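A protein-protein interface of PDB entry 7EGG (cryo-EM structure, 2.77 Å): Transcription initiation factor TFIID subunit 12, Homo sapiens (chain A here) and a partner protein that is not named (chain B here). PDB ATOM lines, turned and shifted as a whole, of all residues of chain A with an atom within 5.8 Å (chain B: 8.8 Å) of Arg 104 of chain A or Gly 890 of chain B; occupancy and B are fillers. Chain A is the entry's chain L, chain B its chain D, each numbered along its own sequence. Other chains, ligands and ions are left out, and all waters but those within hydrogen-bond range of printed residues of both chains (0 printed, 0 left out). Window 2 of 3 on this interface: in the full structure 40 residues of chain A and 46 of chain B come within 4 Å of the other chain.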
ATOM      1  N   ALA A  99     -16.640 -13.317   3.988  1.00  0.00           N
ATOM      2  CA  ALA A  99     -16.039 -12.248   4.799  1.00  0.00           C
ATOM      3  C   ALA A  99     -15.204 -11.376   3.881  1.00  0.00           C
ATOM      4  O   ALA A  99     -15.216 -10.173   4.055  1.00  0.00           O
ATOM      5  CB  ALA A  99     -15.176 -12.900   5.823  1.00  0.00           C
ATOM      6  N   CYS A 100     -14.487 -11.985   2.952  1.00  0.00           N
ATOM      7  CA  CYS A 100     -13.668 -11.256   1.963  1.00  0.00           C
ATOM      8  C   CYS A 100     -14.581 -10.445   1.052  1.00  0.00           C
ATOM      9  O   CYS A 100     -14.215  -9.325   0.723  1.00  0.00           O
ATOM     10  CB  CYS A 100     -12.826 -12.234   1.169  1.00  0.00           C
ATOM     11  SG  CYS A 100     -11.425 -12.883   2.107  1.00  0.00           S
ATOM     12  N   GLN A 101     -15.766 -10.933   0.707  1.00  0.00           N
ATOM     13  CA  GLN A 101     -16.737 -10.141  -0.085  1.00  0.00           C
ATOM     14  C   GLN A 101     -17.164  -8.904   0.701  1.00  0.00           C
ATOM     15  O   GLN A 101     -17.270  -7.847   0.079  1.00  0.00           O
ATOM     16  CB  GLN A 101     -17.933 -11.006  -0.441  1.00  0.00           C
ATOM     17  CG  GLN A 101     -17.609 -12.115  -1.426  1.00  0.00           C
ATOM     18  CD  GLN A 101     -18.822 -12.971  -1.690  1.00  0.00           C
ATOM     19  OE1 GLN A 101     -19.948 -12.482  -1.746  1.00  0.00           O
ATOM     20  NE2 GLN A 101     -18.602 -14.264  -1.851  1.00  0.00           N
ATOM     21  N   LEU A 102     -17.413  -9.026   2.002  1.00  0.00           N
ATOM     22  CA  LEU A 102     -17.754  -7.880   2.883  1.00  0.00           C
ATOM     23  C   LEU A 102     -16.579  -6.916   2.975  1.00  0.00           C
ATOM     24  O   LEU A 102     -16.837  -5.725   3.051  1.00  0.00           O
ATOM     25  CB  LEU A 102     -18.112  -8.392   4.276  1.00  0.00           C
ATOM     26  CG  LEU A 102     -19.195  -9.461   4.347  1.00  0.00           C
ATOM     27  CD1 LEU A 102     -19.604  -9.706   5.785  1.00  0.00           C
ATOM     28  CD2 LEU A 102     -20.397  -9.068   3.516  1.00  0.00           C
ATOM     29  N   ALA A 103     -15.352  -7.411   3.035  1.00  0.00           N
ATOM     30  CA  ALA A 103     -14.142  -6.567   3.121  1.00  0.00           C
ATOM     31  C   ALA A 103     -13.903  -5.797   1.839  1.00  0.00           C
ATOM     32  O   ALA A 103     -13.544  -4.633   1.944  1.00  0.00           O
ATOM     33  CB  ALA A 103     -12.953  -7.408   3.470  1.00  0.00           C
ATOM     34  N   ARG A 104     -14.090  -6.418   0.681  1.00  0.00           N
ATOM     35  CA  ARG A 104     -13.968  -5.675  -0.604  1.00  0.00           C
ATOM     36  C   ARG A 104     -15.055  -4.618  -0.602  1.00  0.00           C
ATOM     37  O   ARG A 104     -14.784  -3.500  -1.019  1.00  0.00           O
ATOM     38  CB  ARG A 104     -14.126  -6.594  -1.812  1.00  0.00           C
ATOM     39  CG  ARG A 104     -13.088  -6.323  -2.888  1.00  0.00           C
ATOM     40  CD  ARG A 104     -11.749  -6.259  -2.184  1.00  0.00           C
ATOM     41  NE  ARG A 104     -10.737  -5.413  -2.794  1.00  0.00           N
ATOM     42  CZ  ARG A 104     -10.632  -4.109  -2.578  1.00  0.00           C
ATOM     43  NH1 ARG A 104      -9.672  -3.417  -3.165  1.00  0.00           N
ATOM     44  NH2 ARG A 104     -11.494  -3.500  -1.783  1.00  0.00           N
ATOM     45  N   HIS A 105     -16.223  -4.959  -0.079  1.00  0.00           N
ATOM     46  CA  HIS A 105     -17.357  -4.014   0.017  1.00  0.00           C
ATOM     47  C   HIS A 105     -16.992  -2.823   0.888  1.00  0.00           C
ATOM     48  O   HIS A 105     -17.420  -1.717   0.550  1.00  0.00           O
ATOM     49  CB  HIS A 105     -18.544  -4.751   0.611  1.00  0.00           C
ATOM     50  CG  HIS A 105     -19.786  -3.943   0.629  1.00  0.00           C
ATOM     51  ND1 HIS A 105     -20.295  -3.421   1.791  1.00  0.00           N
ATOM     52  CD2 HIS A 105     -20.613  -3.571  -0.367  1.00  0.00           C
ATOM     53  CE1 HIS A 105     -21.390  -2.759   1.516  1.00  0.00           C
ATOM     54  NE2 HIS A 105     -21.605  -2.838   0.200  1.00  0.00           N
ATOM     55  N   ARG A 106     -16.235  -3.039   1.953  1.00  0.00           N
ATOM     56  CA  ARG A 106     -15.811  -1.958   2.874  1.00  0.00           C
ATOM     57  C   ARG A 106     -14.563  -1.315   2.263  1.00  0.00           C
ATOM     58  O   ARG A 106     -13.914  -0.523   2.955  1.00  0.00           O
ATOM     59  CB  ARG A 106     -15.568  -2.546   4.266  1.00  0.00           C
ATOM     60  CG  ARG A 106     -14.916  -1.615   5.273  1.00  0.00           C
ATOM     61  CD  ARG A 106     -14.737  -2.405   6.551  1.00  0.00           C
ATOM     62  NE  ARG A 106     -14.010  -3.647   6.330  1.00  0.00           N
ATOM     63  CZ  ARG A 106     -12.731  -3.839   6.637  1.00  0.00           C
ATOM     64  NH1 ARG A 106     -12.156  -5.001   6.389  1.00  0.00           N
ATOM     65  NH2 ARG A 106     -12.025  -2.870   7.188  1.00  0.00           N
ATOM     66  N   LYS A 107     -14.236  -1.663   1.018  1.00  0.00           N
ATOM     67  CA  LYS A 107     -13.061  -1.099   0.304  1.00  0.00           C
ATOM     68  C   LYS A 107     -11.768  -1.349   1.073  1.00  0.00           C
ATOM     69  O   LYS A 107     -11.000  -0.397   1.241  1.00  0.00           O
ATOM     70  CB  LYS A 107     -13.294   0.364  -0.065  1.00  0.00           C
ATOM     71  CG  LYS A 107     -14.525   0.622  -0.920  1.00  0.00           C
ATOM     72  CD  LYS A 107     -14.632  -0.319  -2.096  1.00  0.00           C
ATOM     73  CE  LYS A 107     -16.005  -0.304  -2.730  1.00  0.00           C
ATOM     74  NZ  LYS A 107     -16.411   1.070  -3.109  1.00  0.00           N
ATOM     75  N   SER A 108     -11.538  -2.588   1.514  1.00  0.00           N
ATOM     76  CA  SER A 108     -10.349  -2.875   2.348  1.00  0.00           C
ATOM     77  C   SER A 108      -9.549  -4.056   1.826  1.00  0.00           C
ATOM     78  O   SER A 108     -10.107  -4.880   1.102  1.00  0.00           O
ATOM     79  CB  SER A 108     -10.719  -3.085   3.775  1.00  0.00           C
ATOM     80  OG  SER A 108      -9.886  -2.316   4.627  1.00  0.00           O
ATOM     81  N   SER A 109      -8.260  -4.075   2.140  1.00  0.00           N
ATOM     82  CA  SER A 109      -7.401  -5.225   1.786  1.00  0.00           C
ATOM     83  C   SER A 109      -6.992  -5.918   3.081  1.00  0.00           C
ATOM     84  O   SER A 109      -6.042  -6.695   3.028  1.00  0.00           O
ATOM     85  CB  SER A 109      -6.191  -4.712   1.089  1.00  0.00           C
ATOM     86  OG  SER A 109      -6.560  -3.825   0.046  1.00  0.00           O
ATOM     87  N   LEU B 883      -5.126 -16.782   3.161  1.00  0.00           N
ATOM     88  CA  LEU B 883      -4.480 -15.872   2.221  1.00  0.00           C
ATOM     89  C   LEU B 883      -4.627 -16.324   0.776  1.00  0.00           C
ATOM     90  O   LEU B 883      -4.637 -15.484  -0.128  1.00  0.00           O
ATOM     91  CB  LEU B 883      -2.999 -15.724   2.567  1.00  0.00           C
ATOM     92  CG  LEU B 883      -2.650 -14.792   3.725  1.00  0.00           C
ATOM     93  CD1 LEU B 883      -1.155 -14.803   3.982  1.00  0.00           C
ATOM     94  CD2 LEU B 883      -3.135 -13.384   3.438  1.00  0.00           C
ATOM     95  N   GLU B 884      -4.738 -17.633   0.532  1.00  0.00           N
ATOM     96  CA  GLU B 884      -4.867 -18.106  -0.844  1.00  0.00           C
ATOM     97  C   GLU B 884      -6.261 -17.834  -1.396  1.00  0.00           C
ATOM     98  O   GLU B 884      -6.403 -17.485  -2.575  1.00  0.00           O
ATOM     99  CB  GLU B 884      -4.527 -19.591  -0.937  1.00  0.00           C
ATOM    100  CG  GLU B 884      -4.462 -20.116  -2.368  1.00  0.00           C
ATOM    101  CD  GLU B 884      -4.669 -21.611  -2.462  1.00  0.00           C
ATOM    102  OE1 GLU B 884      -3.700 -22.325  -2.796  1.00  0.00           O
ATOM    103  OE2 GLU B 884      -5.803 -22.076  -2.216  1.00  0.00           O
ATOM    104  N   ILE B 885      -7.297 -17.958  -0.561  1.00  0.00           N
ATOM    105  CA  ILE B 885      -8.633 -17.546  -0.971  1.00  0.00           C
ATOM    106  C   ILE B 885      -8.724 -16.024  -1.077  1.00  0.00           C
ATOM    107  O   ILE B 885      -9.571 -15.497  -1.808  1.00  0.00           O
ATOM    108  CB  ILE B 885      -9.683 -18.111   0.009  1.00  0.00           C
ATOM    109  CG1 ILE B 885      -9.333 -19.543   0.400  1.00  0.00           C
ATOM    110  CG2 ILE B 885     -11.077 -18.097  -0.599  1.00  0.00           C
ATOM    111  CD1 ILE B 885     -10.214 -20.112   1.492  1.00  0.00           C
ATOM    112  N   GLY B 886      -7.846 -15.297  -0.385  1.00  0.00           N
ATOM    113  CA  GLY B 886      -7.830 -13.850  -0.474  1.00  0.00           C
ATOM    114  C   GLY B 886      -7.230 -13.318  -1.754  1.00  0.00           C
ATOM    115  O   GLY B 886      -7.405 -12.134  -2.059  1.00  0.00           O
ATOM    116  N   LYS B 887      -6.515 -14.161  -2.505  1.00  0.00           N
ATOM    117  CA  LYS B 887      -5.989 -13.734  -3.794  1.00  0.00           C
ATOM    118  C   LYS B 887      -7.101 -13.550  -4.816  1.00  0.00           C
ATOM    119  O   LYS B 887      -6.969 -12.730  -5.733  1.00  0.00           O
ATOM    120  CB  LYS B 887      -4.965 -14.744  -4.312  1.00  0.00           C
ATOM    121  CG  LYS B 887      -3.875 -15.117  -3.323  1.00  0.00           C
ATOM    122  CD  LYS B 887      -3.069 -13.908  -2.879  1.00  0.00           C
ATOM    123  CE  LYS B 887      -1.957 -14.315  -1.925  1.00  0.00           C
ATOM    124  NZ  LYS B 887      -1.097 -13.160  -1.556  1.00  0.00           N
ATOM    125  N   LYS B 888      -8.199 -14.292  -4.674  1.00  0.00           N
ATOM    126  CA  LYS B 888      -9.320 -14.204  -5.600  1.00  0.00           C
ATOM    127  C   LYS B 888     -10.204 -12.991  -5.355  1.00  0.00           C
ATOM    128  O   LYS B 888     -11.107 -12.734  -6.157  1.00  0.00           O
ATOM    129  CB  LYS B 888     -10.166 -15.477  -5.517  1.00  0.00           C
ATOM    130  CG  LYS B 888      -9.358 -16.763  -5.493  1.00  0.00           C
ATOM    131  CD  LYS B 888     -10.259 -17.977  -5.650  1.00  0.00           C
ATOM    132  CE  LYS B 888      -9.525 -19.264  -5.309  1.00  0.00           C
ATOM    133  NZ  LYS B 888      -9.290 -19.407  -3.845  1.00  0.00           N
ATOM    134  N   HIS B 889      -9.975 -12.244  -4.274  1.00  0.00           N
ATOM    135  CA  HIS B 889     -10.758 -11.053  -3.988  1.00  0.00           C
ATOM    136  C   HIS B 889      -9.922  -9.798  -3.786  1.00  0.00           C
ATOM    137  O   HIS B 889     -10.482  -8.698  -3.834  1.00  0.00           O
ATOM    138  CB  HIS B 889     -11.632 -11.267  -2.742  1.00  0.00           C
ATOM    139  CG  HIS B 889     -12.473 -12.504  -2.794  1.00  0.00           C
ATOM    140  ND1 HIS B 889     -13.801 -12.484  -3.164  1.00  0.00           N
ATOM    141  CD2 HIS B 889     -12.183 -13.794  -2.508  1.00  0.00           C
ATOM    142  CE1 HIS B 889     -14.288 -13.712  -3.112  1.00  0.00           C
ATOM    143  NE2 HIS B 889     -13.326 -14.525  -2.719  1.00  0.00           N
ATOM    144  N   GLY B 890      -8.614  -9.918  -3.569  1.00  0.00           N
ATOM    145  CA  GLY B 890      -7.772  -8.759  -3.340  1.00  0.00           C
ATOM    146  C   GLY B 890      -7.701  -8.383  -1.876  1.00  0.00           C
ATOM    147  O   GLY B 890      -7.888  -7.221  -1.513  1.00  0.00           O
ATOM    148  N   ILE B 891      -7.446  -9.375  -1.024  1.00  0.00           N
ATOM    149  CA  ILE B 891      -7.496  -9.244   0.430  1.00  0.00           C
ATOM    150  C   ILE B 891      -6.103  -9.605   0.944  1.00  0.00           C
ATOM    151  O   ILE B 891      -5.954 -10.400   1.881  1.00  0.00           O
ATOM    152  CB  ILE B 891      -8.610 -10.115   1.050  1.00  0.00           C
ATOM    153  CG1 ILE B 891      -9.911  -9.981   0.255  1.00  0.00           C
ATOM    154  CG2 ILE B 891      -8.969  -9.637   2.457  1.00  0.00           C
ATOM    155  CD1 ILE B 891     -10.526  -8.582   0.237  1.00  0.00           C
ATOM    156  N   THR B 892      -5.078  -9.088   0.254  1.00  0.00           N
ATOM    157  CA  THR B 892      -3.667  -9.484   0.303  1.00  0.00           C
ATOM    158  C   THR B 892      -3.059  -9.774   1.676  1.00  0.00           C
ATOM    159  O   THR B 892      -2.165 -10.617   1.779  1.00  0.00           O
ATOM    160  CB  THR B 892      -2.818  -8.403  -0.372  1.00  0.00           C
ATOM    161  OG1 THR B 892      -2.677  -7.284   0.512  1.00  0.00           O
ATOM    162  CG2 THR B 892      -3.471  -7.942  -1.668  1.00  0.00           C
ATOM    163  N   GLU B 893      -3.515  -9.107   2.732  1.00  0.00           N
ATOM    164  CA  GLU B 893      -3.061  -9.440   4.076  1.00  0.00           C
ATOM    165  C   GLU B 893      -4.252  -9.465   5.024  1.00  0.00           C
ATOM    166  O   GLU B 893      -5.303  -8.879   4.750  1.00  0.00           O
ATOM    167  CB  GLU B 893      -1.971  -8.470   4.570  1.00  0.00           C
ATOM    168  CG  GLU B 893      -2.376  -7.008   4.687  1.00  0.00           C
ATOM    169  CD  GLU B 893      -2.875  -6.639   6.072  1.00  0.00           C
ATOM    170  OE1 GLU B 893      -2.583  -7.385   7.030  1.00  0.00           O
ATOM    171  OE2 GLU B 893      -3.553  -5.599   6.198  1.00  0.00           O
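Arg 104 of chain A touches just these residues of chain B: His 889, Gly 890 and Ile 891. No residue of chain B comes within 4 Å of Ala 103 of chain A. Of the printed residues of chain A, Thr 892 of chain B touches Ser 109 (3.8 Å). Of the printed residues of chain B, Ser 109 of chain A touches Gly 890 (3.9 Å), Ile 891 (3.6 Å), Thr 892 (3.8 Å) and Glu 893 (2.9 Å). Of the printed residues of chain A, His 889 of chain B touches Cys 100 (3.99 Å) and Arg 104 (3.2 Å). Printed residues of chain A within 4 Å of Glu 893 of chain B: Ser 109 (2.9 Å). Lys 888 of chain B touches none of the printed residues of chain A. The nearest residue of chain B that does not touch Arg 104 of chain A is Gly 886 of chain B (7.3 Å). The nearest residue of chain A that does not touch Gly 890 of chain B is Ser 108 of chain A (4.2 Å). The nearest printed residue of chain B that does not touch Ser 108 of chain A is Gly 890 of chain B (4.2 Å).
Of the 11 printed residues of chain A, 4 touch a printed residue of chain B. Along chain A the printed residues that touch a printed residue of chain B span positions 100 to 109. Printed residues of chain B that touch a printed residue of chain A: His 889, Gly 890, Ile 891, Thr 892 and Glu 893. Hydrophobic or aromatic side chains of chain B within 4 Å of the printed part of chain A: His 889 and Ile 891. Among the printed residues, 10 pairs touch across the chains.
O of Gly 886 of chain B sits at hydrogen-bond distance from N of Ile 891 of chain B (2.9 Å). O of Ala 103 of chain A sits at hydrogen-bond distance from N of Ser 108 of chain A (2.9 Å). The guanidinium group of Arg 104 of chain A is in hydrogen-bond range of the backbone carbonyl oxygen of Ser 108 of chain A (3.5 Å). The side-chain hydroxyl of Ser 108 of chain A is in hydrogen-bond range of the guanidinium group of Arg 106 of chain A, at 3.4 Å.
Among the printed residues, pairs that only touch across the chains: Arg 104 of chain A with Ile 891 of chain B (3.6 Å), Ser 109 of chain A with Ile 891 of chain B (3.6 Å), Arg 104 of chain A with Gly 890 of chain B (3.6 Å), Cys 100 of chain A with Ile 891 of chain B (3.8 Å), Ser 109 of chain A with Thr 892 of chain B (3.8 Å), Ser 108 of chain A with Ile 891 of chain B (3.8 Å), Ser 109 of chain A with Gly 890 of chain B (3.9 Å) and Cys 100 of chain A with His 889 of chain B (3.99 Å).
NE of Arg 104 of chain A sits close to O of His 889 of chain B. The backbone carbonyl oxygen (O) of Ser 109 of chain A lies close to the backbone carbonyl oxygen (O) of Glu 893 of chain B (2.9 Å).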
